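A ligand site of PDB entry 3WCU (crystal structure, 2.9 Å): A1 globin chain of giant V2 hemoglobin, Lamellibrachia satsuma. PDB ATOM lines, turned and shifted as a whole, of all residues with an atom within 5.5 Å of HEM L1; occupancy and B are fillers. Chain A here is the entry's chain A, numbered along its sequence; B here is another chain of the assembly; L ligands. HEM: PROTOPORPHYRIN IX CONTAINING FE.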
ATOM      1  N   TRP A  32     -24.103  -0.349  -1.352  1.00  0.00           N
ATOM      2  CA  TRP A  32     -25.233   0.482  -1.767  1.00  0.00           C
ATOM      3  C   TRP A  32     -25.975   1.146  -0.615  1.00  0.00           C
ATOM      4  O   TRP A  32     -26.534   2.202  -0.784  1.00  0.00           O
ATOM      5  CB  TRP A  32     -26.198  -0.292  -2.644  1.00  0.00           C
ATOM      6  CG  TRP A  32     -25.613  -0.555  -3.971  1.00  0.00           C
ATOM      7  CD1 TRP A  32     -24.821  -1.609  -4.318  1.00  0.00           C
ATOM      8  CD2 TRP A  32     -25.704   0.290  -5.132  1.00  0.00           C
ATOM      9  NE1 TRP A  32     -24.397  -1.474  -5.625  1.00  0.00           N
ATOM     10  CE2 TRP A  32     -24.926  -0.320  -6.148  1.00  0.00           C
ATOM     11  CE3 TRP A  32     -26.348   1.497  -5.417  1.00  0.00           C
ATOM     12  CZ2 TRP A  32     -24.785   0.233  -7.420  1.00  0.00           C
ATOM     13  CZ3 TRP A  32     -26.212   2.055  -6.683  1.00  0.00           C
ATOM     14  CH2 TRP A  32     -25.430   1.414  -7.668  1.00  0.00           C
ATOM     15  N   ALA A  42     -29.289  10.119  -4.782  1.00  0.00           N
ATOM     16  CA  ALA A  42     -28.751   9.160  -5.726  1.00  0.00           C
ATOM     17  C   ALA A  42     -29.689   7.978  -5.987  1.00  0.00           C
ATOM     18  O   ALA A  42     -29.656   7.369  -7.054  1.00  0.00           O
ATOM     19  CB  ALA A  42     -27.402   8.646  -5.242  1.00  0.00           C
ATOM     20  N   LEU A  45     -32.372   7.626  -8.980  1.00  0.00           N
ATOM     21  CA  LEU A  45     -31.791   7.397 -10.293  1.00  0.00           C
ATOM     22  C   LEU A  45     -31.933   5.932 -10.698  1.00  0.00           C
ATOM     23  O   LEU A  45     -31.627   5.562 -11.825  1.00  0.00           O
ATOM     24  CB  LEU A  45     -30.311   7.759 -10.251  1.00  0.00           C
ATOM     25  CG  LEU A  45     -29.990   9.164  -9.750  1.00  0.00           C
ATOM     26  CD1 LEU A  45     -28.522   9.260  -9.389  1.00  0.00           C
ATOM     27  CD2 LEU A  45     -30.369  10.186 -10.820  1.00  0.00           C
ATOM     28  N   PHE A  46     -32.431   5.099  -9.777  1.00  0.00           N
ATOM     29  CA  PHE A  46     -32.566   3.666 -10.039  1.00  0.00           C
ATOM     30  C   PHE A  46     -33.991   3.107  -9.935  1.00  0.00           C
ATOM     31  O   PHE A  46     -34.155   1.911  -9.673  1.00  0.00           O
ATOM     32  CB  PHE A  46     -31.655   2.885  -9.072  1.00  0.00           C
ATOM     33  CG  PHE A  46     -30.192   3.249  -9.183  1.00  0.00           C
ATOM     34  CD1 PHE A  46     -29.402   2.754 -10.221  1.00  0.00           C
ATOM     35  CD2 PHE A  46     -29.590   4.098  -8.248  1.00  0.00           C
ATOM     36  CE1 PHE A  46     -28.066   3.116 -10.321  1.00  0.00           C
ATOM     37  CE2 PHE A  46     -28.261   4.458  -8.354  1.00  0.00           C
ATOM     38  CZ  PHE A  46     -27.501   3.963  -9.389  1.00  0.00           C
ATOM     39  N   SER A  48     -36.041   2.286 -12.130  1.00  0.00           N
ATOM     40  CA  SER A  48     -36.233   1.204 -13.102  1.00  0.00           C
ATOM     41  C   SER A  48     -35.826  -0.189 -12.604  1.00  0.00           C
ATOM     42  O   SER A  48     -36.260  -1.185 -13.162  1.00  0.00           O
ATOM     43  CB  SER A  48     -35.435   1.507 -14.371  1.00  0.00           C
ATOM     44  OG  SER A  48     -34.055   1.624 -14.081  1.00  0.00           O
ATOM     45  N   VAL A  49     -34.996  -0.251 -11.572  1.00  0.00           N
ATOM     46  CA  VAL A  49     -34.581  -1.537 -11.028  1.00  0.00           C
ATOM     47  C   VAL A  49     -35.137  -1.714  -9.617  1.00  0.00           C
ATOM     48  O   VAL A  49     -34.494  -2.288  -8.747  1.00  0.00           O
ATOM     49  CB  VAL A  49     -33.058  -1.648 -10.976  1.00  0.00           C
ATOM     50  CG1 VAL A  49     -32.489  -1.629 -12.385  1.00  0.00           C
ATOM     51  CG2 VAL A  49     -32.485  -0.512 -10.140  1.00  0.00           C
ATOM     52  N   HIS A  62     -29.406  -5.870  -9.543  1.00  0.00           N
ATOM     53  CA  HIS A  62     -28.683  -4.699 -10.045  1.00  0.00           C
ATOM     54  C   HIS A  62     -27.351  -4.634  -9.310  1.00  0.00           C
ATOM     55  O   HIS A  62     -26.301  -4.477  -9.924  1.00  0.00           O
ATOM     56  CB  HIS A  62     -29.477  -3.410  -9.789  1.00  0.00           C
ATOM     57  CG  HIS A  62     -28.712  -2.160 -10.089  1.00  0.00           C
ATOM     58  ND1 HIS A  62     -28.243  -1.844 -11.344  1.00  0.00           N
ATOM     59  CD2 HIS A  62     -28.310  -1.152  -9.276  1.00  0.00           C
ATOM     60  CE1 HIS A  62     -27.593  -0.705 -11.295  1.00  0.00           C
ATOM     61  NE2 HIS A  62     -27.611  -0.253 -10.057  1.00  0.00           N
ATOM     62  N   ARG A  65     -25.092  -6.980 -10.656  1.00  0.00           N
ATOM     63  CA  ARG A  65     -24.579  -6.569 -11.952  1.00  0.00           C
ATOM     64  C   ARG A  65     -23.460  -5.538 -11.877  1.00  0.00           C
ATOM     65  O   ARG A  65     -22.444  -5.669 -12.552  1.00  0.00           O
ATOM     66  CB  ARG A  65     -25.710  -6.023 -12.844  1.00  0.00           C
ATOM     67  CG  ARG A  65     -26.393  -7.087 -13.719  1.00  0.00           C
ATOM     68  CD  ARG A  65     -27.175  -6.428 -14.848  1.00  0.00           C
ATOM     69  NE  ARG A  65     -28.288  -5.643 -14.314  1.00  0.00           N
ATOM     70  CZ  ARG A  65     -29.384  -6.183 -13.789  1.00  0.00           C
ATOM     71  NH1 ARG A  65     -29.507  -7.503 -13.742  1.00  0.00           N
ATOM     72  NH2 ARG A  65     -30.341  -5.399 -13.316  1.00  0.00           N
ATOM     73  N   VAL A  66     -23.646  -4.519 -11.054  1.00  0.00           N
ATOM     74  CA  VAL A  66     -22.673  -3.428 -10.911  1.00  0.00           C
ATOM     75  C   VAL A  66     -21.370  -3.760 -10.219  1.00  0.00           C
ATOM     76  O   VAL A  66     -20.308  -3.660 -10.821  1.00  0.00           O
ATOM     77  CB  VAL A  66     -23.281  -2.225 -10.184  1.00  0.00           C
ATOM     78  CG1 VAL A  66     -22.206  -1.178  -9.918  1.00  0.00           C
ATOM     79  CG2 VAL A  66     -24.399  -1.629 -11.024  1.00  0.00           C
ATOM     80  N   GLY A  69     -19.599  -5.912 -11.949  1.00  0.00           N
ATOM     81  CA  GLY A  69     -18.795  -5.274 -12.961  1.00  0.00           C
ATOM     82  C   GLY A  69     -17.528  -4.743 -12.303  1.00  0.00           C
ATOM     83  O   GLY A  69     -16.416  -4.984 -12.787  1.00  0.00           O
ATOM     84  N   LEU A  70     -17.697  -4.015 -11.207  1.00  0.00           N
ATOM     85  CA  LEU A  70     -16.557  -3.483 -10.492  1.00  0.00           C
ATOM     86  C   LEU A  70     -15.541  -4.594 -10.356  1.00  0.00           C
ATOM     87  O   LEU A  70     -14.351  -4.386 -10.597  1.00  0.00           O
ATOM     88  CB  LEU A  70     -16.967  -3.002  -9.103  1.00  0.00           C
ATOM     89  CG  LEU A  70     -16.190  -1.800  -8.605  1.00  0.00           C
ATOM     90  CD1 LEU A  70     -16.168  -1.788  -7.091  1.00  0.00           C
ATOM     91  CD2 LEU A  70     -14.775  -1.846  -9.144  1.00  0.00           C
ATOM     92  N   ARG A  72     -15.016  -7.346 -12.250  1.00  0.00           N
ATOM     93  CA  ARG A  72     -14.301  -7.614 -13.496  1.00  0.00           C
ATOM     94  C   ARG A  72     -13.345  -6.495 -13.857  1.00  0.00           C
ATOM     95  O   ARG A  72     -12.182  -6.752 -14.194  1.00  0.00           O
ATOM     96  CB  ARG A  72     -15.274  -7.867 -14.655  1.00  0.00           C
ATOM     97  CG  ARG A  72     -15.780  -6.651 -15.392  1.00  0.00           C
ATOM     98  CD  ARG A  72     -16.407  -7.114 -16.689  1.00  0.00           C
ATOM     99  NE  ARG A  72     -17.037  -6.043 -17.453  1.00  0.00           N
ATOM    100  CZ  ARG A  72     -18.200  -5.469 -17.147  1.00  0.00           C
ATOM    101  NH1 ARG A  72     -18.877  -5.877 -16.081  1.00  0.00           N
ATOM    102  NH2 ARG A  72     -18.703  -4.518 -17.929  1.00  0.00           N
ATOM    103  N   VAL A  73     -13.810  -5.254 -13.798  1.00  0.00           N
ATOM    104  CA  VAL A  73     -12.937  -4.136 -14.123  1.00  0.00           C
ATOM    105  C   VAL A  73     -11.642  -4.263 -13.306  1.00  0.00           C
ATOM    106  O   VAL A  73     -10.565  -4.483 -13.876  1.00  0.00           O
ATOM    107  CB  VAL A  73     -13.641  -2.793 -13.828  1.00  0.00           C
ATOM    108  CG1 VAL A  73     -12.683  -1.633 -14.074  1.00  0.00           C
ATOM    109  CG2 VAL A  73     -14.843  -2.658 -14.727  1.00  0.00           C
ATOM    110  N   LEU A  90     -18.111   0.364 -21.089  1.00  0.00           N
ATOM    111  CA  LEU A  90     -19.002   0.818 -20.031  1.00  0.00           C
ATOM    112  C   LEU A  90     -19.382   2.272 -20.242  1.00  0.00           C
ATOM    113  O   LEU A  90     -20.511   2.667 -19.959  1.00  0.00           O
ATOM    114  CB  LEU A  90     -18.322   0.674 -18.661  1.00  0.00           C
ATOM    115  CG  LEU A  90     -18.322  -0.708 -18.010  1.00  0.00           C
ATOM    116  CD1 LEU A  90     -17.312  -0.729 -16.871  1.00  0.00           C
ATOM    117  CD2 LEU A  90     -19.719  -1.048 -17.509  1.00  0.00           C
ATOM    118  N   GLN A  93     -22.304   2.493 -22.322  1.00  0.00           N
ATOM    119  CA  GLN A  93     -23.504   2.011 -21.669  1.00  0.00           C
ATOM    120  C   GLN A  93     -23.980   3.060 -20.661  1.00  0.00           C
ATOM    121  O   GLN A  93     -25.177   3.223 -20.422  1.00  0.00           O
ATOM    122  CB  GLN A  93     -23.234   0.668 -20.970  1.00  0.00           C
ATOM    123  CG  GLN A  93     -22.694  -0.431 -21.888  1.00  0.00           C
ATOM    124  CD  GLN A  93     -22.623  -1.796 -21.230  1.00  0.00           C
ATOM    125  OE1 GLN A  93     -22.026  -1.969 -20.164  1.00  0.00           O
ATOM    126  NE2 GLN A  93     -23.221  -2.782 -21.859  1.00  0.00           N
ATOM    127  N   HIS A  94     -23.056   3.800 -20.075  1.00  0.00           N
ATOM    128  CA  HIS A  94     -23.442   4.800 -19.101  1.00  0.00           C
ATOM    129  C   HIS A  94     -23.644   6.206 -19.674  1.00  0.00           C
ATOM    130  O   HIS A  94     -24.428   6.981 -19.123  1.00  0.00           O
ATOM    131  CB  HIS A  94     -22.433   4.852 -17.961  1.00  0.00           C
ATOM    132  CG  HIS A  94     -22.611   3.765 -16.933  1.00  0.00           C
ATOM    133  ND1 HIS A  94     -21.994   2.536 -17.034  1.00  0.00           N
ATOM    134  CD2 HIS A  94     -23.315   3.743 -15.769  1.00  0.00           C
ATOM    135  CE1 HIS A  94     -22.317   1.806 -15.983  1.00  0.00           C
ATOM    136  NE2 HIS A  94     -23.114   2.505 -15.196  1.00  0.00           N
ATOM    137  N   ARG A  97     -27.195   7.484 -20.043  1.00  0.00           N
ATOM    138  CA  ARG A  97     -27.968   7.607 -18.810  1.00  0.00           C
ATOM    139  C   ARG A  97     -27.884   9.036 -18.313  1.00  0.00           C
ATOM    140  O   ARG A  97     -28.627   9.431 -17.422  1.00  0.00           O
ATOM    141  CB  ARG A  97     -27.442   6.656 -17.725  1.00  0.00           C
ATOM    142  CG  ARG A  97     -28.030   5.256 -17.781  1.00  0.00           C
ATOM    143  CD  ARG A  97     -26.929   4.222 -17.778  1.00  0.00           C
ATOM    144  NE  ARG A  97     -27.459   2.900 -18.061  1.00  0.00           N
ATOM    145  CZ  ARG A  97     -26.700   1.821 -18.238  1.00  0.00           C
ATOM    146  NH1 ARG A  97     -25.375   1.910 -18.175  1.00  0.00           N
ATOM    147  NH2 ARG A  97     -27.267   0.648 -18.490  1.00  0.00           N
ATOM    148  N   LEU A  99     -25.602  10.731 -16.444  1.00  0.00           N
ATOM    149  CA  LEU A  99     -25.370  10.699 -14.999  1.00  0.00           C
ATOM    150  C   LEU A  99     -24.346  11.714 -14.525  1.00  0.00           C
ATOM    151  O   LEU A  99     -23.223  11.800 -15.055  1.00  0.00           O
ATOM    152  CB  LEU A  99     -24.873   9.305 -14.578  1.00  0.00           C
ATOM    153  CG  LEU A  99     -25.689   8.079 -14.994  1.00  0.00           C
ATOM    154  CD1 LEU A  99     -24.769   6.879 -15.088  1.00  0.00           C
ATOM    155  CD2 LEU A  99     -26.824   7.860 -14.014  1.00  0.00           C
ATOM    156  N   ASN A 103     -21.895  11.437  -8.546  1.00  0.00           N
ATOM    157  CA  ASN A 103     -22.268  10.190  -7.882  1.00  0.00           C
ATOM    158  C   ASN A 103     -21.087   9.220  -7.973  1.00  0.00           C
ATOM    159  O   ASN A 103     -20.814   8.449  -7.045  1.00  0.00           O
ATOM    160  CB  ASN A 103     -23.489   9.589  -8.534  1.00  0.00           C
ATOM    161  CG  ASN A 103     -24.633  10.570  -8.631  1.00  0.00           C
ATOM    162  OD1 ASN A 103     -24.914  11.082  -9.703  1.00  0.00           O
ATOM    163  ND2 ASN A 103     -25.301  10.838  -7.505  1.00  0.00           N
ATOM    164  N   PHE A 104     -20.391   9.244  -9.096  1.00  0.00           N
ATOM    165  CA  PHE A 104     -19.239   8.372  -9.219  1.00  0.00           C
ATOM    166  C   PHE A 104     -18.227   8.677  -8.116  1.00  0.00           C
ATOM    167  O   PHE A 104     -17.367   7.848  -7.803  1.00  0.00           O
ATOM    168  CB  PHE A 104     -18.616   8.525 -10.594  1.00  0.00           C
ATOM    169  CG  PHE A 104     -19.308   7.715 -11.635  1.00  0.00           C
ATOM    170  CD1 PHE A 104     -18.877   6.444 -11.931  1.00  0.00           C
ATOM    171  CD2 PHE A 104     -20.424   8.208 -12.299  1.00  0.00           C
ATOM    172  CE1 PHE A 104     -19.525   5.666 -12.872  1.00  0.00           C
ATOM    173  CE2 PHE A 104     -21.088   7.446 -13.240  1.00  0.00           C
ATOM    174  CZ  PHE A 104     -20.639   6.164 -13.525  1.00  0.00           C
ATOM    175  N   PHE A 107     -19.742   6.764  -5.194  1.00  0.00           N
ATOM    176  CA  PHE A 107     -19.499   5.342  -5.377  1.00  0.00           C
ATOM    177  C   PHE A 107     -18.071   5.063  -4.940  1.00  0.00           C
ATOM    178  O   PHE A 107     -17.742   3.950  -4.516  1.00  0.00           O
ATOM    179  CB  PHE A 107     -19.698   4.938  -6.836  1.00  0.00           C
ATOM    180  CG  PHE A 107     -19.602   3.465  -7.084  1.00  0.00           C
ATOM    181  CD1 PHE A 107     -18.395   2.795  -6.950  1.00  0.00           C
ATOM    182  CD2 PHE A 107     -20.724   2.747  -7.469  1.00  0.00           C
ATOM    183  CE1 PHE A 107     -18.302   1.437  -7.187  1.00  0.00           C
ATOM    184  CE2 PHE A 107     -20.638   1.387  -7.712  1.00  0.00           C
ATOM    185  CZ  PHE A 107     -19.427   0.732  -7.570  1.00  0.00           C
ATOM    186  N   TYR A 132      -8.962   3.908  -8.523  1.00  0.00           N
ATOM    187  CA  TYR A 132     -10.394   3.992  -8.759  1.00  0.00           C
ATOM    188  C   TYR A 132     -10.640   5.204  -9.633  1.00  0.00           C
ATOM    189  O   TYR A 132     -11.618   5.260 -10.360  1.00  0.00           O
ATOM    190  CB  TYR A 132     -11.163   4.132  -7.454  1.00  0.00           C
ATOM    191  CG  TYR A 132     -12.587   4.537  -7.668  1.00  0.00           C
ATOM    192  CD1 TYR A 132     -12.968   5.865  -7.537  1.00  0.00           C
ATOM    193  CD2 TYR A 132     -13.536   3.607  -8.077  1.00  0.00           C
ATOM    194  CE1 TYR A 132     -14.252   6.267  -7.825  1.00  0.00           C
ATOM    195  CE2 TYR A 132     -14.824   3.993  -8.355  1.00  0.00           C
ATOM    196  CZ  TYR A 132     -15.186   5.333  -8.234  1.00  0.00           C
ATOM    197  OH  TYR A 132     -16.452   5.743  -8.561  1.00  0.00           O
ATOM    198  N   ILE A 135     -10.843   4.027 -13.029  1.00  0.00           N
ATOM    199  CA  ILE A 135     -12.125   3.462 -13.441  1.00  0.00           C
ATOM    200  C   ILE A 135     -13.164   4.558 -13.719  1.00  0.00           C
ATOM    201  O   ILE A 135     -13.925   4.462 -14.676  1.00  0.00           O
ATOM    202  CB  ILE A 135     -12.663   2.483 -12.381  1.00  0.00           C
ATOM    203  CG1 ILE A 135     -11.705   1.305 -12.226  1.00  0.00           C
ATOM    204  CG2 ILE A 135     -14.039   1.975 -12.786  1.00  0.00           C
ATOM    205  CD1 ILE A 135     -12.017   0.422 -11.062  1.00  0.00           C
ATOM    206  N   ILE A 139     -14.959   5.583 -17.201  1.00  0.00           N
ATOM    207  CA  ILE A 139     -16.401   5.490 -17.357  1.00  0.00           C
ATOM    208  C   ILE A 139     -17.044   6.852 -17.580  1.00  0.00           C
ATOM    209  O   ILE A 139     -17.727   7.063 -18.583  1.00  0.00           O
ATOM    210  CB  ILE A 139     -17.039   4.806 -16.126  1.00  0.00           C
ATOM    211  CG1 ILE A 139     -16.733   3.307 -16.179  1.00  0.00           C
ATOM    212  CG2 ILE A 139     -18.545   5.079 -16.073  1.00  0.00           C
ATOM    213  CD1 ILE A 139     -17.380   2.481 -15.097  1.00  0.00           C
ATOM    214  N   HIS B  94     -32.623 -11.162 -17.181  1.00  0.00           N
ATOM    215  CA  HIS B  94     -31.978  -9.984 -17.732  1.00  0.00           C
ATOM    216  C   HIS B  94     -30.979 -10.403 -18.816  1.00  0.00           C
ATOM    217  O   HIS B  94     -30.881  -9.757 -19.865  1.00  0.00           O
ATOM    218  CB  HIS B  94     -31.277  -9.238 -16.611  1.00  0.00           C
ATOM    219  CG  HIS B  94     -31.072  -7.784 -16.878  1.00  0.00           C
ATOM    220  ND1 HIS B  94     -30.167  -7.319 -17.804  1.00  0.00           N
ATOM    221  CD2 HIS B  94     -31.650  -6.689 -16.323  1.00  0.00           C
ATOM    222  CE1 HIS B  94     -30.199  -5.995 -17.824  1.00  0.00           C
ATOM    223  NE2 HIS B  94     -31.087  -5.591 -16.934  1.00  0.00           N
ATOM    224  N   GLN B  98     -31.130  -9.930 -23.326  1.00  0.00           N
ATOM    225  CA  GLN B  98     -30.029  -9.442 -24.146  1.00  0.00           C
ATOM    226  C   GLN B  98     -29.583 -10.426 -25.225  1.00  0.00           C
ATOM    227  O   GLN B  98     -29.509 -10.067 -26.393  1.00  0.00           O
ATOM    228  CB  GLN B  98     -28.834  -9.087 -23.272  1.00  0.00           C
ATOM    229  CG  GLN B  98     -29.211  -8.213 -22.096  1.00  0.00           C
ATOM    230  CD  GLN B  98     -28.016  -7.762 -21.305  1.00  0.00           C
ATOM    231  OE1 GLN B  98     -27.052  -8.524 -21.130  1.00  0.00           O
ATOM    232  NE2 GLN B  98     -28.063  -6.527 -20.801  1.00  0.00           N
HETATM  233  CHA HEM L   1     -26.158  -0.008 -15.029  1.00  0.00           C
HETATM  234  CHB HEM L   1     -21.668  -1.030 -13.932  1.00  0.00           C
HETATM  235  CHC HEM L   1     -21.299   3.077 -11.395  1.00  0.00           C
HETATM  236  CHD HEM L   1     -25.837   4.083 -12.589  1.00  0.00           C
HETATM  237  C1A HEM L   1     -24.970  -0.669 -14.953  1.00  0.00           C
HETATM  238  C2A HEM L   1     -24.757  -1.924 -15.527  1.00  0.00           C
HETATM  239  C3A HEM L   1     -23.467  -2.230 -15.234  1.00  0.00           C
HETATM  240  C4A HEM L   1     -22.892  -1.140 -14.456  1.00  0.00           C
HETATM  241  CMA HEM L   1     -22.676  -3.487 -15.603  1.00  0.00           C
HETATM  242  CAA HEM L   1     -25.821  -2.724 -16.295  1.00  0.00           C
HETATM  243  CBA HEM L   1     -25.443  -3.452 -17.549  1.00  0.00           C
HETATM  244  CGA HEM L   1     -26.621  -4.228 -18.169  1.00  0.00           C
HETATM  245  O1A HEM L   1     -27.798  -3.743 -18.129  1.00  0.00           O
HETATM  246  O2A HEM L   1     -26.394  -5.305 -18.654  1.00  0.00           O
HETATM  247  C1B HEM L   1     -21.130   0.013 -13.131  1.00  0.00           C
HETATM  248  C2B HEM L   1     -19.784   0.011 -12.589  1.00  0.00           C
HETATM  249  C3B HEM L   1     -19.698   1.241 -11.833  1.00  0.00           C
HETATM  250  C4B HEM L   1     -20.956   1.862 -11.975  1.00  0.00           C
HETATM  251  CMB HEM L   1     -18.751  -1.043 -12.783  1.00  0.00           C
HETATM  252  CAB HEM L   1     -18.528   1.654 -11.100  1.00  0.00           C
HETATM  253  CBB HEM L   1     -17.346   1.887 -11.634  1.00  0.00           C
HETATM  254  C1C HEM L   1     -22.540   3.708 -11.511  1.00  0.00           C
HETATM  255  C2C HEM L   1     -22.850   4.990 -10.859  1.00  0.00           C
HETATM  256  C3C HEM L   1     -24.170   5.315 -11.197  1.00  0.00           C
HETATM  257  C4C HEM L   1     -24.609   4.156 -12.063  1.00  0.00           C
HETATM  258  CMC HEM L   1     -21.902   5.804  -9.985  1.00  0.00           C
HETATM  259  CAC HEM L   1     -24.888   6.400 -10.820  1.00  0.00           C
HETATM  260  CBC HEM L   1     -25.719   6.773  -9.912  1.00  0.00           C
HETATM  261  C1D HEM L   1     -26.332   3.063 -13.368  1.00  0.00           C
HETATM  262  C2D HEM L   1     -27.735   3.022 -13.912  1.00  0.00           C
HETATM  263  C3D HEM L   1     -27.805   1.848 -14.602  1.00  0.00           C
HETATM  264  C4D HEM L   1     -26.483   1.193 -14.484  1.00  0.00           C
HETATM  265  CMD HEM L   1     -28.795   4.109 -13.674  1.00  0.00           C
HETATM  266  CAD HEM L   1     -29.006   1.283 -15.348  1.00  0.00           C
HETATM  267  CBD HEM L   1     -29.752   0.281 -14.522  1.00  0.00           C
HETATM  268  CGD HEM L   1     -30.918  -0.310 -15.209  1.00  0.00           C
HETATM  269  O1D HEM L   1     -32.002   0.331 -15.264  1.00  0.00           O
HETATM  270  O2D HEM L   1     -30.812  -1.450 -15.724  1.00  0.00           O
HETATM  271  NA  HEM L   1     -23.840  -0.172 -14.283  1.00  0.00           N
HETATM  272  NB  HEM L   1     -21.834   1.088 -12.783  1.00  0.00           N
HETATM  273  NC  HEM L   1     -23.635   3.254 -12.233  1.00  0.00           N
HETATM  274  ND  HEM L   1     -25.625   1.969 -13.747  1.00  0.00           N
HETATM  275 FE   HEM L   1     -23.727   1.560 -13.282  1.00  0.00          FE
HETATM  276  CHA HEM L   2     -22.657 -10.582 -24.750  1.00  0.00           C
HETATM  277  CHB HEM L   2     -22.698 -13.452 -20.966  1.00  0.00           C
HETATM  278  CHC HEM L   2     -22.917 -17.356 -23.817  1.00  0.00           C
HETATM  279  CHD HEM L   2     -22.983 -14.428 -27.641  1.00  0.00           C
HETATM  280  C1A HEM L   2     -22.639 -11.020 -23.441  1.00  0.00           C
HETATM  281  C2A HEM L   2     -22.529 -10.152 -22.344  1.00  0.00           C
HETATM  282  C3A HEM L   2     -22.555 -10.950 -21.272  1.00  0.00           C
HETATM  283  C4A HEM L   2     -22.668 -12.347 -21.710  1.00  0.00           C
HETATM  284  CMA HEM L   2     -22.449 -10.512 -19.802  1.00  0.00           C
HETATM  285  CAA HEM L   2     -22.376  -8.655 -22.336  1.00  0.00           C
HETATM  286  CBA HEM L   2     -23.574  -7.808 -22.468  1.00  0.00           C
HETATM  287  CGA HEM L   2     -23.159  -6.320 -22.459  1.00  0.00           C
HETATM  288  O1A HEM L   2     -22.458  -5.872 -23.421  1.00  0.00           O
HETATM  289  O2A HEM L   2     -23.483  -5.631 -21.515  1.00  0.00           O
HETATM  290  C1B HEM L   2     -22.751 -14.822 -21.386  1.00  0.00           C
HETATM  291  C2B HEM L   2     -22.741 -15.954 -20.481  1.00  0.00           C
HETATM  292  C3B HEM L   2     -22.793 -17.107 -21.354  1.00  0.00           C
HETATM  293  C4B HEM L   2     -22.849 -16.576 -22.668  1.00  0.00           C
HETATM  294  CMB HEM L   2     -22.665 -15.912 -18.990  1.00  0.00           C
HETATM  295  CAB HEM L   2     -22.785 -18.477 -20.887  1.00  0.00           C
HETATM  296  CBB HEM L   2     -23.778 -19.060 -20.257  1.00  0.00           C
HETATM  297  C1C HEM L   2     -22.967 -16.877 -25.112  1.00  0.00           C
HETATM  298  C2C HEM L   2     -23.045 -17.768 -26.273  1.00  0.00           C
HETATM  299  C3C HEM L   2     -23.070 -16.946 -27.415  1.00  0.00           C
HETATM  300  C4C HEM L   2     -22.999 -15.534 -26.851  1.00  0.00           C
HETATM  301  CMC HEM L   2     -23.077 -19.300 -26.215  1.00  0.00           C
HETATM  302  CAC HEM L   2     -23.142 -17.333 -28.715  1.00  0.00           C
HETATM  303  CBC HEM L   2     -22.424 -17.933 -29.600  1.00  0.00           C
HETATM  304  C1D HEM L   2     -22.897 -13.120 -27.186  1.00  0.00           C
HETATM  305  C2D HEM L   2     -22.848 -11.912 -28.115  1.00  0.00           C
HETATM  306  C3D HEM L   2     -22.751 -10.812 -27.268  1.00  0.00           C
HETATM  307  C4D HEM L   2     -22.752 -11.356 -25.883  1.00  0.00           C
HETATM  308  CMD HEM L   2     -22.896 -11.989 -29.631  1.00  0.00           C
HETATM  309  CAD HEM L   2     -22.661  -9.331 -27.654  1.00  0.00           C
HETATM  310  CBD HEM L   2     -21.224  -8.888 -27.892  1.00  0.00           C
HETATM  311  CGD HEM L   2     -21.043  -7.445 -28.254  1.00  0.00           C
HETATM  312  O1D HEM L   2     -21.557  -6.541 -27.518  1.00  0.00           O
HETATM  313  O2D HEM L   2     -20.376  -7.141 -29.256  1.00  0.00           O
HETATM  314  NA  HEM L   2     -22.722 -12.381 -23.070  1.00  0.00           N
HETATM  315  NB  HEM L   2     -22.816 -15.158 -22.674  1.00  0.00           N
HETATM  316  NC  HEM L   2     -22.951 -15.544 -25.506  1.00  0.00           N
HETATM  317  ND  HEM L   2     -22.829 -12.747 -25.893  1.00  0.00           N
HETATM  318 FE   HEM L   2     -22.854 -13.973 -24.296  1.00  0.00          FE
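FE of HEM L1 is bound by NE2 of His 94 of chain A (2.2 Å).
The side-chain hydroxyl (OG) of Ser 48 sits at hydrogen-bond distance from an oxygen (O1D) of HEM L1 (2.7 Å).
The side-chain amide nitrogen (NE2) of Gln 98 of chain B lies within hydrogen-bond range of an oxygen (O2A) of HEM L1 (3.0 Å).
The side-chain amide nitrogen of Gln 93 sits at hydrogen-bond distance from an oxygen (O2A) of HEM L2 (2.9 Å).
Merely in contact with HEM L1: Leu 45 (3.7 Å), Phe 46 (3.3 Å), Val 49 (3.5 Å), His 62 (3.9 Å), Arg 65 (3.8 Å), Val 66 (3.6 Å), Gly 69 (3.9 Å), Leu 70 (3.5 Å), Arg 97 (3.5 Å), Leu 99 (3.9 Å), Asn 103 (3.8 Å), Phe 104 (3.5 Å), Phe 107 (3.8 Å), Ile 135 (3.5 Å), Ile 139 (3.5 Å) and His 94 of chain B (3.3 Å).
Hydrophobic or aromatic side chains within 4 Å of HEM L1: Leu 45, Phe 46, Val 49, His 62, Val 66, His 94 of chain A, Leu 99, Phe 104, Phe 107, Ile 135, Ile 139 and His 94 of chain B.
Within 4 Å of HEM L1: Leu 45, Phe 46, Ser 48, Val 49, His 62, Arg 65, Val 66, Gly 69, Leu 70, His 94 of chain A, Arg 97, Leu 99, Asn 103, Phe 104, Phe 107, Ile 135, Ile 139, His 94 of chain B and Gln 98 of chain B.
The nearest printed residue that does not touch HEM L1 is Leu 90 (4.1 Å).
ND1 of His 94 of chain A sits at hydrogen-bond distance from O of Leu 90.
O of Phe 104 lies within hydrogen-bond range of OH of Tyr 132 (2.4 Å).
The guanidinium group of Arg 97 lies within hydrogen-bond range of the backbone carbonyl oxygen of Gln 93 (2.6 Å).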
